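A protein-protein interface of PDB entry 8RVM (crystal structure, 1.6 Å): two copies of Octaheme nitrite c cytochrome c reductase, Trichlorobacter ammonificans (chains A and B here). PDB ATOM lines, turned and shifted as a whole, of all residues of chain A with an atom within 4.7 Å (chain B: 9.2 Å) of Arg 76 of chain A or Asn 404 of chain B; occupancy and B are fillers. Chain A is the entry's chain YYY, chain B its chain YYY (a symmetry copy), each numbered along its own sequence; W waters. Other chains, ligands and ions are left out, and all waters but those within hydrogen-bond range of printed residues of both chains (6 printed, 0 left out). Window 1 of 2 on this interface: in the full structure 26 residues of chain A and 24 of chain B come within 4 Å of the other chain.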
ATOM      1  N   THR A  73     -20.395  -4.846  12.564  1.00  0.00           N
ATOM      2  CA  THR A  73     -20.094  -4.124  11.289  1.00  0.00           C
ATOM      3  C   THR A  73     -21.271  -4.294  10.333  1.00  0.00           C
ATOM      4  O   THR A  73     -21.207  -3.767   9.255  1.00  0.00           O
ATOM      5  CB  THR A  73     -18.786  -4.612  10.669  1.00  0.00           C
ATOM      6  OG1 THR A  73     -18.937  -5.975  10.247  1.00  0.00           O
ATOM      7  CG2 THR A  73     -17.614  -4.416  11.616  1.00  0.00           C
ATOM      8  N   GLY A  74     -22.300  -5.029  10.734  1.00  0.00           N
ATOM      9  CA  GLY A  74     -23.522  -5.195   9.937  1.00  0.00           C
ATOM     10  C   GLY A  74     -23.355  -6.249   8.864  1.00  0.00           C
ATOM     11  O   GLY A  74     -22.281  -6.888   8.758  1.00  0.00           O
ATOM     12  N   ALA A  75     -24.394  -6.382   8.059  1.00  0.00           N
ATOM     13  CA  ALA A  75     -24.474  -7.312   6.923  1.00  0.00           C
ATOM     14  C   ALA A  75     -24.906  -6.536   5.688  1.00  0.00           C
ATOM     15  O   ALA A  75     -24.908  -5.298   5.701  1.00  0.00           O
ATOM     16  CB  ALA A  75     -25.435  -8.431   7.257  1.00  0.00           C
ATOM     17  N   ARG A  76     -25.295  -7.269   4.659  1.00  0.00           N
ATOM     18  CA  ARG A  76     -25.644  -6.659   3.356  1.00  0.00           C
ATOM     19  C   ARG A  76     -24.500  -5.758   2.872  1.00  0.00           C
ATOM     20  O   ARG A  76     -24.769  -4.666   2.270  1.00  0.00           O
ATOM     21  CB  ARG A  76     -27.002  -5.969   3.466  1.00  0.00           C
ATOM     22  CG  ARG A  76     -27.660  -5.851   2.104  1.00  0.00           C
ATOM     23  CD  ARG A  76     -29.005  -6.489   1.998  1.00  0.00           C
ATOM     24  NE  ARG A  76     -29.551  -6.281   0.652  1.00  0.00           N
ATOM     25  CZ  ARG A  76     -30.831  -6.429   0.361  1.00  0.00           C
ATOM     26  NH1 ARG A  76     -31.672  -6.803   1.310  1.00  0.00           N
ATOM     27  NH2 ARG A  76     -31.267  -6.213  -0.876  1.00  0.00           N
ATOM     28  N   LYS A  77     -23.264  -6.239   3.053  1.00  0.00           N
ATOM     29  CA  LYS A  77     -22.034  -5.521   2.625  1.00  0.00           C
ATOM     30  C   LYS A  77     -21.875  -5.663   1.120  1.00  0.00           C
ATOM     31  O   LYS A  77     -21.439  -6.709   0.652  1.00  0.00           O
ATOM     32  CB  LYS A  77     -20.804  -6.075   3.343  1.00  0.00           C
ATOM     33  CG  LYS A  77     -20.893  -5.879   4.858  1.00  0.00           C
ATOM     34  CD  LYS A  77     -19.688  -6.422   5.555  1.00  0.00           C
ATOM     35  CE  LYS A  77     -19.685  -6.209   7.063  1.00  0.00           C
ATOM     36  NZ  LYS A  77     -18.617  -7.041   7.663  1.00  0.00           N
ATOM     37  N   GLU A  78     -22.183  -4.603   0.400  1.00  0.00           N
ATOM     38  CA  GLU A  78     -21.948  -4.552  -1.063  1.00  0.00           C
ATOM     39  C   GLU A  78     -20.448  -4.721  -1.314  1.00  0.00           C
ATOM     40  O   GLU A  78     -19.611  -4.006  -0.670  1.00  0.00           O
ATOM     41  CB  GLU A  78     -22.586  -3.261  -1.586  1.00  0.00           C
ATOM     42  CG  GLU A  78     -22.291  -2.978  -3.055  1.00  0.00           C
ATOM     43  CD  GLU A  78     -22.702  -4.056  -4.052  1.00  0.00           C
ATOM     44  OE1 GLU A  78     -23.877  -4.544  -3.985  1.00  0.00           O
ATOM     45  OE2 GLU A  78     -21.831  -4.379  -4.921  1.00  0.00           O
ATOM     46  N   GLU A 101     -26.652  -5.725  -7.429  1.00  0.00           N
ATOM     47  CA  GLU A 101     -26.295  -5.916  -5.994  1.00  0.00           C
ATOM     48  C   GLU A 101     -25.543  -7.226  -5.848  1.00  0.00           C
ATOM     49  O   GLU A 101     -26.008  -8.277  -6.363  1.00  0.00           O
ATOM     50  CB  GLU A 101     -27.481  -5.911  -5.040  1.00  0.00           C
ATOM     51  CG  GLU A 101     -27.050  -6.111  -3.583  1.00  0.00           C
ATOM     52  CD  GLU A 101     -28.175  -5.984  -2.573  1.00  0.00           C
ATOM     53  OE1 GLU A 101     -29.373  -6.073  -2.988  1.00  0.00           O
ATOM     54  OE2 GLU A 101     -27.852  -5.823  -1.376  1.00  0.00           O
ATOM     55  N   ALA A 103     -23.590  -8.747  -2.354  1.00  0.00           N
ATOM     56  CA  ALA A 103     -23.105  -8.529  -0.975  1.00  0.00           C
ATOM     57  C   ALA A 103     -22.288  -9.730  -0.527  1.00  0.00           C
ATOM     58  O   ALA A 103     -22.425 -10.824  -1.086  1.00  0.00           O
ATOM     59  CB  ALA A 103     -24.238  -8.288  -0.020  1.00  0.00           C
ATOM     60  N   ALA A 117     -34.358 -11.897  -1.505  1.00  0.00           N
ATOM     61  CA  ALA A 117     -34.493 -10.443  -1.232  1.00  0.00           C
ATOM     62  C   ALA A 117     -33.442  -9.625  -1.981  1.00  0.00           C
ATOM     63  O   ALA A 117     -33.614  -8.384  -2.090  1.00  0.00           O
ATOM     64  CB  ALA A 117     -34.392 -10.181   0.246  1.00  0.00           C
ATOM     65  N   VAL A 118     -32.377 -10.245  -2.465  1.00  0.00           N
ATOM     66  CA  VAL A 118     -31.269  -9.478  -3.106  1.00  0.00           C
ATOM     67  C   VAL A 118     -31.843  -8.732  -4.319  1.00  0.00           C
ATOM     68  O   VAL A 118     -32.775  -9.245  -4.973  1.00  0.00           O
ATOM     69  CB  VAL A 118     -30.057 -10.359  -3.487  1.00  0.00           C
ATOM     70  CG1 VAL A 118     -30.342 -11.264  -4.669  1.00  0.00           C
ATOM     71  CG2 VAL A 118     -28.807  -9.532  -3.753  1.00  0.00           C
ATOM     72  N   ASP A 119     -31.296  -7.558  -4.606  1.00  0.00           N
ATOM     73  CA  ASP A 119     -31.851  -6.671  -5.660  1.00  0.00           C
ATOM     74  C   ASP A 119     -31.720  -7.336  -7.023  1.00  0.00           C
ATOM     75  O   ASP A 119     -32.416  -6.869  -7.927  1.00  0.00           O
ATOM     76  CB  ASP A 119     -31.176  -5.319  -5.684  1.00  0.00           C
ATOM     77  CG  ASP A 119     -31.572  -4.435  -4.521  1.00  0.00           C
ATOM     78  OD1 ASP A 119     -32.511  -4.798  -3.790  1.00  0.00           O
ATOM     79  OD2 ASP A 119     -30.923  -3.406  -4.375  1.00  0.00           O
ATOM     80  N   TRP A 132     -35.999  -3.485   7.739  1.00  0.00           N
ATOM     81  CA  TRP A 132     -34.638  -3.645   8.312  1.00  0.00           C
ATOM     82  C   TRP A 132     -34.681  -4.177   9.740  1.00  0.00           C
ATOM     83  O   TRP A 132     -33.749  -4.885  10.125  1.00  0.00           O
ATOM     84  CB  TRP A 132     -33.869  -2.330   8.287  1.00  0.00           C
ATOM     85  CG  TRP A 132     -33.447  -1.988   6.904  1.00  0.00           C
ATOM     86  CD1 TRP A 132     -33.853  -0.920   6.164  1.00  0.00           C
ATOM     87  CD2 TRP A 132     -32.577  -2.769   6.073  1.00  0.00           C
ATOM     88  NE1 TRP A 132     -33.228  -0.940   4.956  1.00  0.00           N
ATOM     89  CE2 TRP A 132     -32.487  -2.087   4.845  1.00  0.00           C
ATOM     90  CE3 TRP A 132     -31.858  -3.950   6.248  1.00  0.00           C
ATOM     91  CZ2 TRP A 132     -31.685  -2.549   3.804  1.00  0.00           C
ATOM     92  CZ3 TRP A 132     -31.104  -4.430   5.205  1.00  0.00           C
ATOM     93  CH2 TRP A 132     -31.024  -3.739   3.994  1.00  0.00           C
ATOM     94  N   TYR A 135     -34.256  -7.822   9.797  1.00  0.00           N
ATOM     95  CA  TYR A 135     -33.248  -8.370   8.854  1.00  0.00           C
ATOM     96  C   TYR A 135     -32.456  -9.509   9.513  1.00  0.00           C
ATOM     97  O   TYR A 135     -31.864 -10.323   8.789  1.00  0.00           O
ATOM     98  CB  TYR A 135     -32.325  -7.264   8.334  1.00  0.00           C
ATOM     99  CG  TYR A 135     -31.410  -7.734   7.236  1.00  0.00           C
ATOM    100  CD1 TYR A 135     -31.928  -8.002   5.991  1.00  0.00           C
ATOM    101  CD2 TYR A 135     -30.034  -7.821   7.401  1.00  0.00           C
ATOM    102  CE1 TYR A 135     -31.115  -8.381   4.944  1.00  0.00           C
ATOM    103  CE2 TYR A 135     -29.204  -8.207   6.361  1.00  0.00           C
ATOM    104  CZ  TYR A 135     -29.754  -8.472   5.126  1.00  0.00           C
ATOM    105  OH  TYR A 135     -28.984  -8.864   4.099  1.00  0.00           O
ATOM    106  N   LYS B 396     -25.694  -2.022  16.911  1.00  0.00           N
ATOM    107  CA  LYS B 396     -24.596  -1.734  15.958  1.00  0.00           C
ATOM    108  C   LYS B 396     -24.920  -2.412  14.622  1.00  0.00           C
ATOM    109  O   LYS B 396     -24.778  -1.786  13.564  1.00  0.00           O
ATOM    110  CB  LYS B 396     -23.283  -2.200  16.554  1.00  0.00           C
ATOM    111  CG  LYS B 396     -22.838  -1.355  17.738  1.00  0.00           C
ATOM    112  CD  LYS B 396     -21.617  -1.918  18.443  1.00  0.00           C
ATOM    113  CE  LYS B 396     -21.228  -1.076  19.633  1.00  0.00           C
ATOM    114  NZ  LYS B 396     -20.073  -1.641  20.367  1.00  0.00           N
ATOM    115  N   PHE B 397     -25.306  -3.684  14.655  1.00  0.00           N
ATOM    116  CA  PHE B 397     -25.653  -4.428  13.418  1.00  0.00           C
ATOM    117  C   PHE B 397     -26.761  -3.689  12.659  1.00  0.00           C
ATOM    118  O   PHE B 397     -26.705  -3.574  11.404  1.00  0.00           O
ATOM    119  CB  PHE B 397     -26.056  -5.849  13.803  1.00  0.00           C
ATOM    120  CG  PHE B 397     -26.699  -6.595  12.673  1.00  0.00           C
ATOM    121  CD1 PHE B 397     -25.933  -7.431  11.886  1.00  0.00           C
ATOM    122  CD2 PHE B 397     -28.054  -6.499  12.431  1.00  0.00           C
ATOM    123  CE1 PHE B 397     -26.521  -8.146  10.856  1.00  0.00           C
ATOM    124  CE2 PHE B 397     -28.640  -7.247  11.426  1.00  0.00           C
ATOM    125  CZ  PHE B 397     -27.863  -8.065  10.626  1.00  0.00           C
ATOM    126  N   MET B 398     -27.767  -3.162  13.345  1.00  0.00           N
ATOM    127  CA  MET B 398     -28.920  -2.519  12.672  1.00  0.00           C
ATOM    128  C   MET B 398     -28.464  -1.211  12.019  1.00  0.00           C
ATOM    129  O   MET B 398     -28.704  -1.031  10.821  1.00  0.00           O
ATOM    130  CB  MET B 398     -30.065  -2.284  13.649  1.00  0.00           C
ATOM    131  CG  MET B 398     -30.827  -3.562  13.985  1.00  0.00           C
ATOM    132  SD  MET B 398     -31.572  -4.261  12.507  1.00  0.00           S
ATOM    133  CE  MET B 398     -32.138  -5.864  13.061  1.00  0.00           C
ATOM    134  N   ILE B 399     -27.700  -0.413  12.740  1.00  0.00           N
ATOM    135  CA  ILE B 399     -27.168   0.857  12.184  1.00  0.00           C
ATOM    136  C   ILE B 399     -26.314   0.505  10.978  1.00  0.00           C
ATOM    137  O   ILE B 399     -26.495   1.121   9.935  1.00  0.00           O
ATOM    138  CB  ILE B 399     -26.344   1.654  13.197  1.00  0.00           C
ATOM    139  CG1 ILE B 399     -27.175   2.039  14.419  1.00  0.00           C
ATOM    140  CG2 ILE B 399     -25.759   2.874  12.502  1.00  0.00           C
ATOM    141  CD1 ILE B 399     -26.312   2.535  15.580  1.00  0.00           C
ATOM    142  N   GLU B 400     -25.391  -0.422  11.139  1.00  0.00           N
ATOM    143  CA  GLU B 400     -24.343  -0.605  10.117  1.00  0.00           C
ATOM    144  C   GLU B 400     -24.909  -1.353   8.925  1.00  0.00           C
ATOM    145  O   GLU B 400     -24.421  -1.029   7.804  1.00  0.00           O
ATOM    146  CB  GLU B 400     -23.137  -1.332  10.709  1.00  0.00           C
ATOM    147  CG  GLU B 400     -22.347  -0.476  11.642  1.00  0.00           C
ATOM    148  CD  GLU B 400     -21.660   0.762  11.071  1.00  0.00           C
ATOM    149  OE1 GLU B 400     -21.939   1.174   9.910  1.00  0.00           O
ATOM    150  OE2 GLU B 400     -20.848   1.322  11.790  1.00  0.00           O
ATOM    151  N   THR B 401     -25.914  -2.219   9.108  1.00  0.00           N
ATOM    152  CA  THR B 401     -26.533  -2.922   7.951  1.00  0.00           C
ATOM    153  C   THR B 401     -27.194  -1.872   7.059  1.00  0.00           C
ATOM    154  O   THR B 401     -27.051  -1.930   5.795  1.00  0.00           O
ATOM    155  CB  THR B 401     -27.503  -4.022   8.403  1.00  0.00           C
ATOM    156  OG1 THR B 401     -26.734  -5.021   9.061  1.00  0.00           O
ATOM    157  CG2 THR B 401     -28.235  -4.626   7.224  1.00  0.00           C
ATOM    158  N   ILE B 402     -27.926  -0.934   7.644  1.00  0.00           N
ATOM    159  CA  ILE B 402     -28.638   0.087   6.843  1.00  0.00           C
ATOM    160  C   ILE B 402     -27.600   0.960   6.113  1.00  0.00           C
ATOM    161  O   ILE B 402     -27.812   1.273   4.937  1.00  0.00           O
ATOM    162  CB  ILE B 402     -29.585   0.921   7.713  1.00  0.00           C
ATOM    163  CG1 ILE B 402     -30.762   0.053   8.170  1.00  0.00           C
ATOM    164  CG2 ILE B 402     -29.998   2.154   6.905  1.00  0.00           C
ATOM    165  CD1 ILE B 402     -31.531   0.602   9.348  1.00  0.00           C
ATOM    166  N   ARG B 403     -26.543   1.360   6.830  1.00  0.00           N
ATOM    167  CA  ARG B 403     -25.475   2.215   6.295  1.00  0.00           C
ATOM    168  C   ARG B 403     -24.802   1.420   5.179  1.00  0.00           C
ATOM    169  O   ARG B 403     -24.506   2.001   4.105  1.00  0.00           O
ATOM    170  CB  ARG B 403     -24.536   2.711   7.389  1.00  0.00           C
ATOM    171  CG  ARG B 403     -25.161   3.760   8.298  1.00  0.00           C
ATOM    172  CD  ARG B 403     -24.138   4.716   8.876  1.00  0.00           C
ATOM    173  NE  ARG B 403     -23.154   4.029   9.684  1.00  0.00           N
ATOM    174  CZ  ARG B 403     -22.232   4.662  10.364  1.00  0.00           C
ATOM    175  NH1 ARG B 403     -21.372   3.996  11.123  1.00  0.00           N
ATOM    176  NH2 ARG B 403     -22.222   5.977  10.331  1.00  0.00           N
ATOM    177  N   ASN B 404     -24.616   0.123   5.384  1.00  0.00           N
ATOM    178  CA  ASN B 404     -23.935  -0.763   4.422  1.00  0.00           C
ATOM    179  C   ASN B 404     -24.734  -0.767   3.111  1.00  0.00           C
ATOM    180  O   ASN B 404     -24.130  -0.521   2.060  1.00  0.00           O
ATOM    181  CB  ASN B 404     -23.831  -2.199   4.972  1.00  0.00           C
ATOM    182  CG  ASN B 404     -22.690  -2.368   5.956  1.00  0.00           C
ATOM    183  OD1 ASN B 404     -21.772  -1.525   6.070  1.00  0.00           O
ATOM    184  ND2 ASN B 404     -22.736  -3.488   6.678  1.00  0.00           N
ATOM    185  N   TYR B 405     -26.025  -1.053   3.189  1.00  0.00           N
ATOM    186  CA  TYR B 405     -26.880  -1.155   1.988  1.00  0.00           C
ATOM    187  C   TYR B 405     -26.937   0.221   1.319  1.00  0.00           C
ATOM    188  O   TYR B 405     -26.803   0.301   0.105  1.00  0.00           O
ATOM    189  CB  TYR B 405     -28.280  -1.622   2.329  1.00  0.00           C
ATOM    190  CG  TYR B 405     -29.152  -1.744   1.115  1.00  0.00           C
ATOM    191  CD1 TYR B 405     -28.951  -2.775   0.223  1.00  0.00           C
ATOM    192  CD2 TYR B 405     -30.133  -0.812   0.835  1.00  0.00           C
ATOM    193  CE1 TYR B 405     -29.734  -2.913  -0.910  1.00  0.00           C
ATOM    194  CE2 TYR B 405     -30.939  -0.944  -0.280  1.00  0.00           C
ATOM    195  CZ  TYR B 405     -30.723  -1.980  -1.165  1.00  0.00           C
ATOM    196  OH  TYR B 405     -31.522  -2.101  -2.259  1.00  0.00           O
ATOM    197  N   THR B 406     -27.098   1.267   2.102  1.00  0.00           N
ATOM    198  CA  THR B 406     -27.220   2.661   1.557  1.00  0.00           C
ATOM    199  C   THR B 406     -25.905   3.076   0.876  1.00  0.00           C
ATOM    200  O   THR B 406     -25.932   3.540  -0.301  1.00  0.00           O
ATOM    201  CB  THR B 406     -27.651   3.656   2.629  1.00  0.00           C
ATOM    202  OG1 THR B 406     -28.875   3.224   3.224  1.00  0.00           O
ATOM    203  CG2 THR B 406     -27.846   5.019   2.002  1.00  0.00           C
ATOM    204  N   LYS B 407     -24.776   2.839   1.523  1.00  0.00           N
ATOM    205  CA  LYS B 407     -23.438   3.168   0.960  1.00  0.00           C
ATOM    206  C   LYS B 407     -23.187   2.380  -0.318  1.00  0.00           C
ATOM    207  O   LYS B 407     -22.603   2.980  -1.284  1.00  0.00           O
ATOM    208  CB  LYS B 407     -22.353   2.969   2.007  1.00  0.00           C
ATOM    209  CG  LYS B 407     -22.447   4.025   3.084  1.00  0.00           C
ATOM    210  CD  LYS B 407     -21.261   4.046   3.966  1.00  0.00           C
ATOM    211  CE  LYS B 407     -21.301   2.884   4.913  1.00  0.00           C
ATOM    212  NZ  LYS B 407     -20.096   2.907   5.772  1.00  0.00           N
ATOM    213  N   GLY B 408     -23.645   1.132  -0.390  1.00  0.00           N
ATOM    214  CA  GLY B 408     -23.509   0.364  -1.634  1.00  0.00           C
ATOM    215  C   GLY B 408     -24.133   1.148  -2.795  1.00  0.00           C
ATOM    216  O   GLY B 408     -23.505   1.212  -3.893  1.00  0.00           O
ATOM    217  N   LYS B 409     -25.311   1.730  -2.560  1.00  0.00           N
ATOM    218  CA  LYS B 409     -26.048   2.492  -3.619  1.00  0.00           C
ATOM    219  C   LYS B 409     -25.387   3.853  -3.789  1.00  0.00           C
ATOM    220  O   LYS B 409     -25.343   4.370  -4.927  1.00  0.00           O
ATOM    221  CB  LYS B 409     -27.531   2.572  -3.274  1.00  0.00           C
ATOM    222  CG  LYS B 409     -28.212   1.234  -3.120  1.00  0.00           C
ATOM    223  CD  LYS B 409     -28.018   0.255  -4.272  1.00  0.00           C
ATOM    224  CE  LYS B 409     -28.799  -1.006  -4.009  1.00  0.00           C
ATOM    225  NZ  LYS B 409     -28.594  -2.031  -5.022  1.00  0.00           N
ATOM    226  N   MET B 410     -24.902   4.475  -2.718  1.00  0.00           N
ATOM    227  CA  MET B 410     -24.197   5.776  -2.848  1.00  0.00           C
ATOM    228  C   MET B 410     -22.965   5.594  -3.751  1.00  0.00           C
ATOM    229  O   MET B 410     -22.724   6.442  -4.683  1.00  0.00           O
ATOM    230  CB  MET B 410     -23.776   6.304  -1.478  1.00  0.00           C
ATOM    231  CG  MET B 410     -24.983   6.658  -0.629  1.00  0.00           C
ATOM    232  SD  MET B 410     -24.501   7.087   1.087  1.00  0.00           S
ATOM    233  CE  MET B 410     -23.653   8.623   0.713  1.00  0.00           C
ATOM    234  N   ARG B 411     -22.165   4.554  -3.493  1.00  0.00           N
ATOM    235  CA  ARG B 411     -20.903   4.323  -4.235  1.00  0.00           C
ATOM    236  C   ARG B 411     -21.276   4.023  -5.697  1.00  0.00           C
ATOM    237  O   ARG B 411     -20.603   4.540  -6.605  1.00  0.00           O
ATOM    238  CB  ARG B 411     -20.090   3.183  -3.617  1.00  0.00           C
ATOM    239  CG  ARG B 411     -19.626   3.439  -2.183  1.00  0.00           C
ATOM    240  CD  ARG B 411     -18.703   4.605  -1.933  1.00  0.00           C
ATOM    241  NE  ARG B 411     -19.333   5.929  -1.881  1.00  0.00           N
ATOM    242  CZ  ARG B 411     -19.784   6.514  -0.775  1.00  0.00           C
ATOM    243  NH1 ARG B 411     -20.342   7.709  -0.811  1.00  0.00           N
ATOM    244  NH2 ARG B 411     -19.740   5.854   0.381  1.00  0.00           N
ATOM    245  N   LYS B 412     -22.358   3.285  -5.917  1.00  0.00           N
ATOM    246  CA  LYS B 412     -22.780   2.897  -7.292  1.00  0.00           C
ATOM    247  C   LYS B 412     -23.263   4.163  -7.999  1.00  0.00           C
ATOM    248  O   LYS B 412     -22.929   4.356  -9.214  1.00  0.00           O
ATOM    249  CB  LYS B 412     -23.847   1.810  -7.247  1.00  0.00           C
ATOM    250  CG  LYS B 412     -24.119   1.093  -8.563  1.00  0.00           C
ATOM    251  CD  LYS B 412     -25.168  -0.026  -8.415  1.00  0.00           C
ATOM    252  CE  LYS B 412     -24.763  -1.104  -7.420  1.00  0.00           C
ATOM    253  NZ  LYS B 412     -23.450  -1.684  -7.827  1.00  0.00           N
ATOM    254  N   SER B 459     -26.125  10.605   7.889  1.00  0.00           N
ATOM    255  CA  SER B 459     -26.515   9.293   8.466  1.00  0.00           C
ATOM    256  C   SER B 459     -26.215   8.135   7.530  1.00  0.00           C
ATOM    257  O   SER B 459     -26.473   7.001   7.946  1.00  0.00           O
ATOM    258  CB  SER B 459     -27.944   9.275   8.891  1.00  0.00           C
ATOM    259  OG  SER B 459     -28.816   9.222   7.788  1.00  0.00           O
ATOM    260  N   ASP B 460     -25.794   8.378   6.289  1.00  0.00           N
ATOM    261  CA  ASP B 460     -25.671   7.284   5.285  1.00  0.00           C
ATOM    262  C   ASP B 460     -26.924   6.394   5.268  1.00  0.00           C
ATOM    263  O   ASP B 460     -26.808   5.159   5.214  1.00  0.00           O
ATOM    264  CB  ASP B 460     -24.410   6.464   5.489  1.00  0.00           C
ATOM    265  CG  ASP B 460     -23.153   7.241   5.191  1.00  0.00           C
ATOM    266  OD1 ASP B 460     -23.065   7.725   4.041  1.00  0.00           O
ATOM    267  OD2 ASP B 460     -22.299   7.378   6.125  1.00  0.00           O
ATOM    268  N   GLY B 461     -28.085   7.026   5.283  1.00  0.00           N
ATOM    269  CA  GLY B 461     -29.392   6.399   5.082  1.00  0.00           C
ATOM    270  C   GLY B 461     -30.120   6.035   6.366  1.00  0.00           C
ATOM    271  O   GLY B 461     -31.333   5.748   6.288  1.00  0.00           O
ATOM    272  N   PHE B 462     -29.429   6.006   7.494  1.00  0.00           N
ATOM    273  CA  PHE B 462     -30.080   5.534   8.734  1.00  0.00           C
ATOM    274  C   PHE B 462     -31.351   6.343   8.963  1.00  0.00           C
ATOM    275  O   PHE B 462     -32.375   5.790   9.328  1.00  0.00           O
ATOM    276  CB  PHE B 462     -29.179   5.576   9.954  1.00  0.00           C
ATOM    277  CG  PHE B 462     -29.857   4.950  11.152  1.00  0.00           C
ATOM    278  CD1 PHE B 462     -29.878   3.578  11.289  1.00  0.00           C
ATOM    279  CD2 PHE B 462     -30.581   5.717  12.055  1.00  0.00           C
ATOM    280  CE1 PHE B 462     -30.538   2.972  12.356  1.00  0.00           C
ATOM    281  CE2 PHE B 462     -31.271   5.115  13.101  1.00  0.00           C
ATOM    282  CZ  PHE B 462     -31.228   3.739  13.257  1.00  0.00           C
ATOM    283  N   ARG B 469     -32.858   4.869  -0.706  1.00  0.00           N
ATOM    284  CA  ARG B 469     -32.819   3.862  -1.785  1.00  0.00           C
ATOM    285  C   ARG B 469     -33.502   4.487  -3.016  1.00  0.00           C
ATOM    286  O   ARG B 469     -32.932   4.419  -4.133  1.00  0.00           O
ATOM    287  CB  ARG B 469     -33.436   2.518  -1.393  1.00  0.00           C
ATOM    288  CG  ARG B 469     -33.229   1.458  -2.471  1.00  0.00           C
ATOM    289  CD  ARG B 469     -34.074   0.195  -2.425  1.00  0.00           C
ATOM    290  NE  ARG B 469     -33.463  -0.717  -3.387  1.00  0.00           N
ATOM    291  CZ  ARG B 469     -33.648  -0.651  -4.721  1.00  0.00           C
ATOM    292  NH1 ARG B 469     -34.524   0.198  -5.225  1.00  0.00           N
ATOM    293  NH2 ARG B 469     -32.966  -1.447  -5.526  1.00  0.00           N
ATOM    294  N   LEU B 472     -31.178   7.285  -4.467  1.00  0.00           N
ATOM    295  CA  LEU B 472     -29.884   6.858  -5.033  1.00  0.00           C
ATOM    296  C   LEU B 472     -30.110   5.976  -6.264  1.00  0.00           C
ATOM    297  O   LEU B 472     -29.372   6.141  -7.257  1.00  0.00           O
ATOM    298  CB  LEU B 472     -29.080   6.156  -3.946  1.00  0.00           C
ATOM    299  CG  LEU B 472     -28.613   7.115  -2.868  1.00  0.00           C
ATOM    300  CD1 LEU B 472     -28.184   6.336  -1.639  1.00  0.00           C
ATOM    301  CD2 LEU B 472     -27.516   8.025  -3.367  1.00  0.00           C
HETATM  302  O   HOH W   1     -21.767  -1.833   1.671  1.00  0.00           O
HETATM  303  O   HOH W   2     -19.703  -1.921   8.083  1.00  0.00           O
HETATM  304  O   HOH W   3     -21.041  -2.957  -7.382  1.00  0.00           O
HETATM  305  O   HOH W   4     -25.781  -2.630  -4.210  1.00  0.00           O
HETATM  306  O   HOH W   5     -23.390  -4.475  -7.151  1.00  0.00           O
HETATM  307  O   HOH W   6     -33.899  -3.863  -1.399  1.00  0.00           O
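O of Trp 132 of chain A sits close to SD of Met 398 of chain B (3.3 Å). OD2 of Asp 119 of chain A is in salt-bridge range of NZ of Lys 409 of chain B, at 2.8 Å. O of Thr 73 of chain A lies within hydrogen-bond range of ND2 of Asn 404 of chain B (3.0 Å). The backbone carbonyl oxygen (O) of Ala 75 of chain A lies within hydrogen-bond range of the side-chain amide nitrogen (ND2) of Asn 404 of chain B, at 3.0 Å. OD2 of Asp 119 of chain A lies within salt-bridge range of NH2 of Arg 469 of chain B (3.1 Å). The side-chain carboxylate (OD2) of Asp 119 of chain A sits at hydrogen-bond distance from the side-chain hydroxyl (OH) of Tyr 405 of chain B (2.6 Å). OG1 of Thr 401 of chain B is in hydrogen-bond range of N of Ala 75 of chain A (2.9 Å).
NE of Arg 76 of chain A lies within salt-bridge range of OE2 of Glu 101 of chain A (2.7 Å). OG1 of Thr 73 of chain A sits at hydrogen-bond distance from NZ of Lys 77 of chain A (2.8 Å). O of Glu 400 of chain B lies close to ND2 of Asn 404 of chain B, at 3.2 Å.
Among the printed residues, pairs that only touch across the chains: Gly 74 of chain A with Thr 401 of chain B, Thr 73 of chain A with Glu 400 of chain B, Glu 101 of chain A with Tyr 405 of chain B, Trp 132 of chain A with Thr 401 of chain B, Lys 77 of chain A with Asn 404 of chain B, Gly 74 of chain A with Asn 404 of chain B, Arg 76 of chain A with Tyr 405 of chain B, Trp 132 of chain A with Ile 402 of chain B, Tyr 135 of chain A with Thr 401 of chain B, Glu 78 of chain A with Gly 408 of chain B, Ala 75 of chain A with Phe 397 of chain B, Trp 132 of chain A with Tyr 405 of chain B, Arg 76 of chain A with Asn 404 of chain B, Gly 74 of chain A with Glu 400 of chain B, Gly 74 of chain A with Phe 397 of chain B and Tyr 135 of chain A with Phe 397 of chain B.
Gly 74 of chain A touches four residues of chain B. Ala 75 of chain A touches just these residues of chain B: Phe 397 (3.8 Å), Thr 401 (2.9 Å) and Asn 404 (3.0 Å). Of the printed residues of chain A, Ile 402 of chain B touches Trp 132. Of chain A, only Thr 73, Gly 74, Ala 75, Arg 76 and Lys 77 come within 4 Å of Asn 404 of chain B. Arg 411 of chain B touches none of the printed residues of chain A. Of the printed residues of chain A, Arg 469 of chain B touches Asp 119 (3.1 Å).
Printed residues of chain A that touch a printed residue of chain B: Thr 73, Gly 74, Ala 75, Arg 76, Lys 77, Glu 78, Glu 101, Asp 119, Trp 132 and Tyr 135. Hydrophobic or aromatic side chains of chain A that line the printed part of chain B: Ala 75, Trp 132 and Tyr 135. Among the printed residues, Asp or Glu carboxylates within 4 Å of a Lys or Arg side-chain nitrogen of the other chain: Asp 119 of chain A with Lys 409 of chain B and Asp 119 of chain A with Arg 469 of chain B.
No position is printed for both chains.
Water W5 bridges the side-chain carboxylate (OE2) of Glu 78 of chain A and the side-chain amino group (NZ) of Lys 412 of chain B. Water W3 lies within hydrogen-bond range of NZ of Lys 412 of chain B (2.8 Å) and OE2 of Glu 78 of chain A (3.0 Å).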
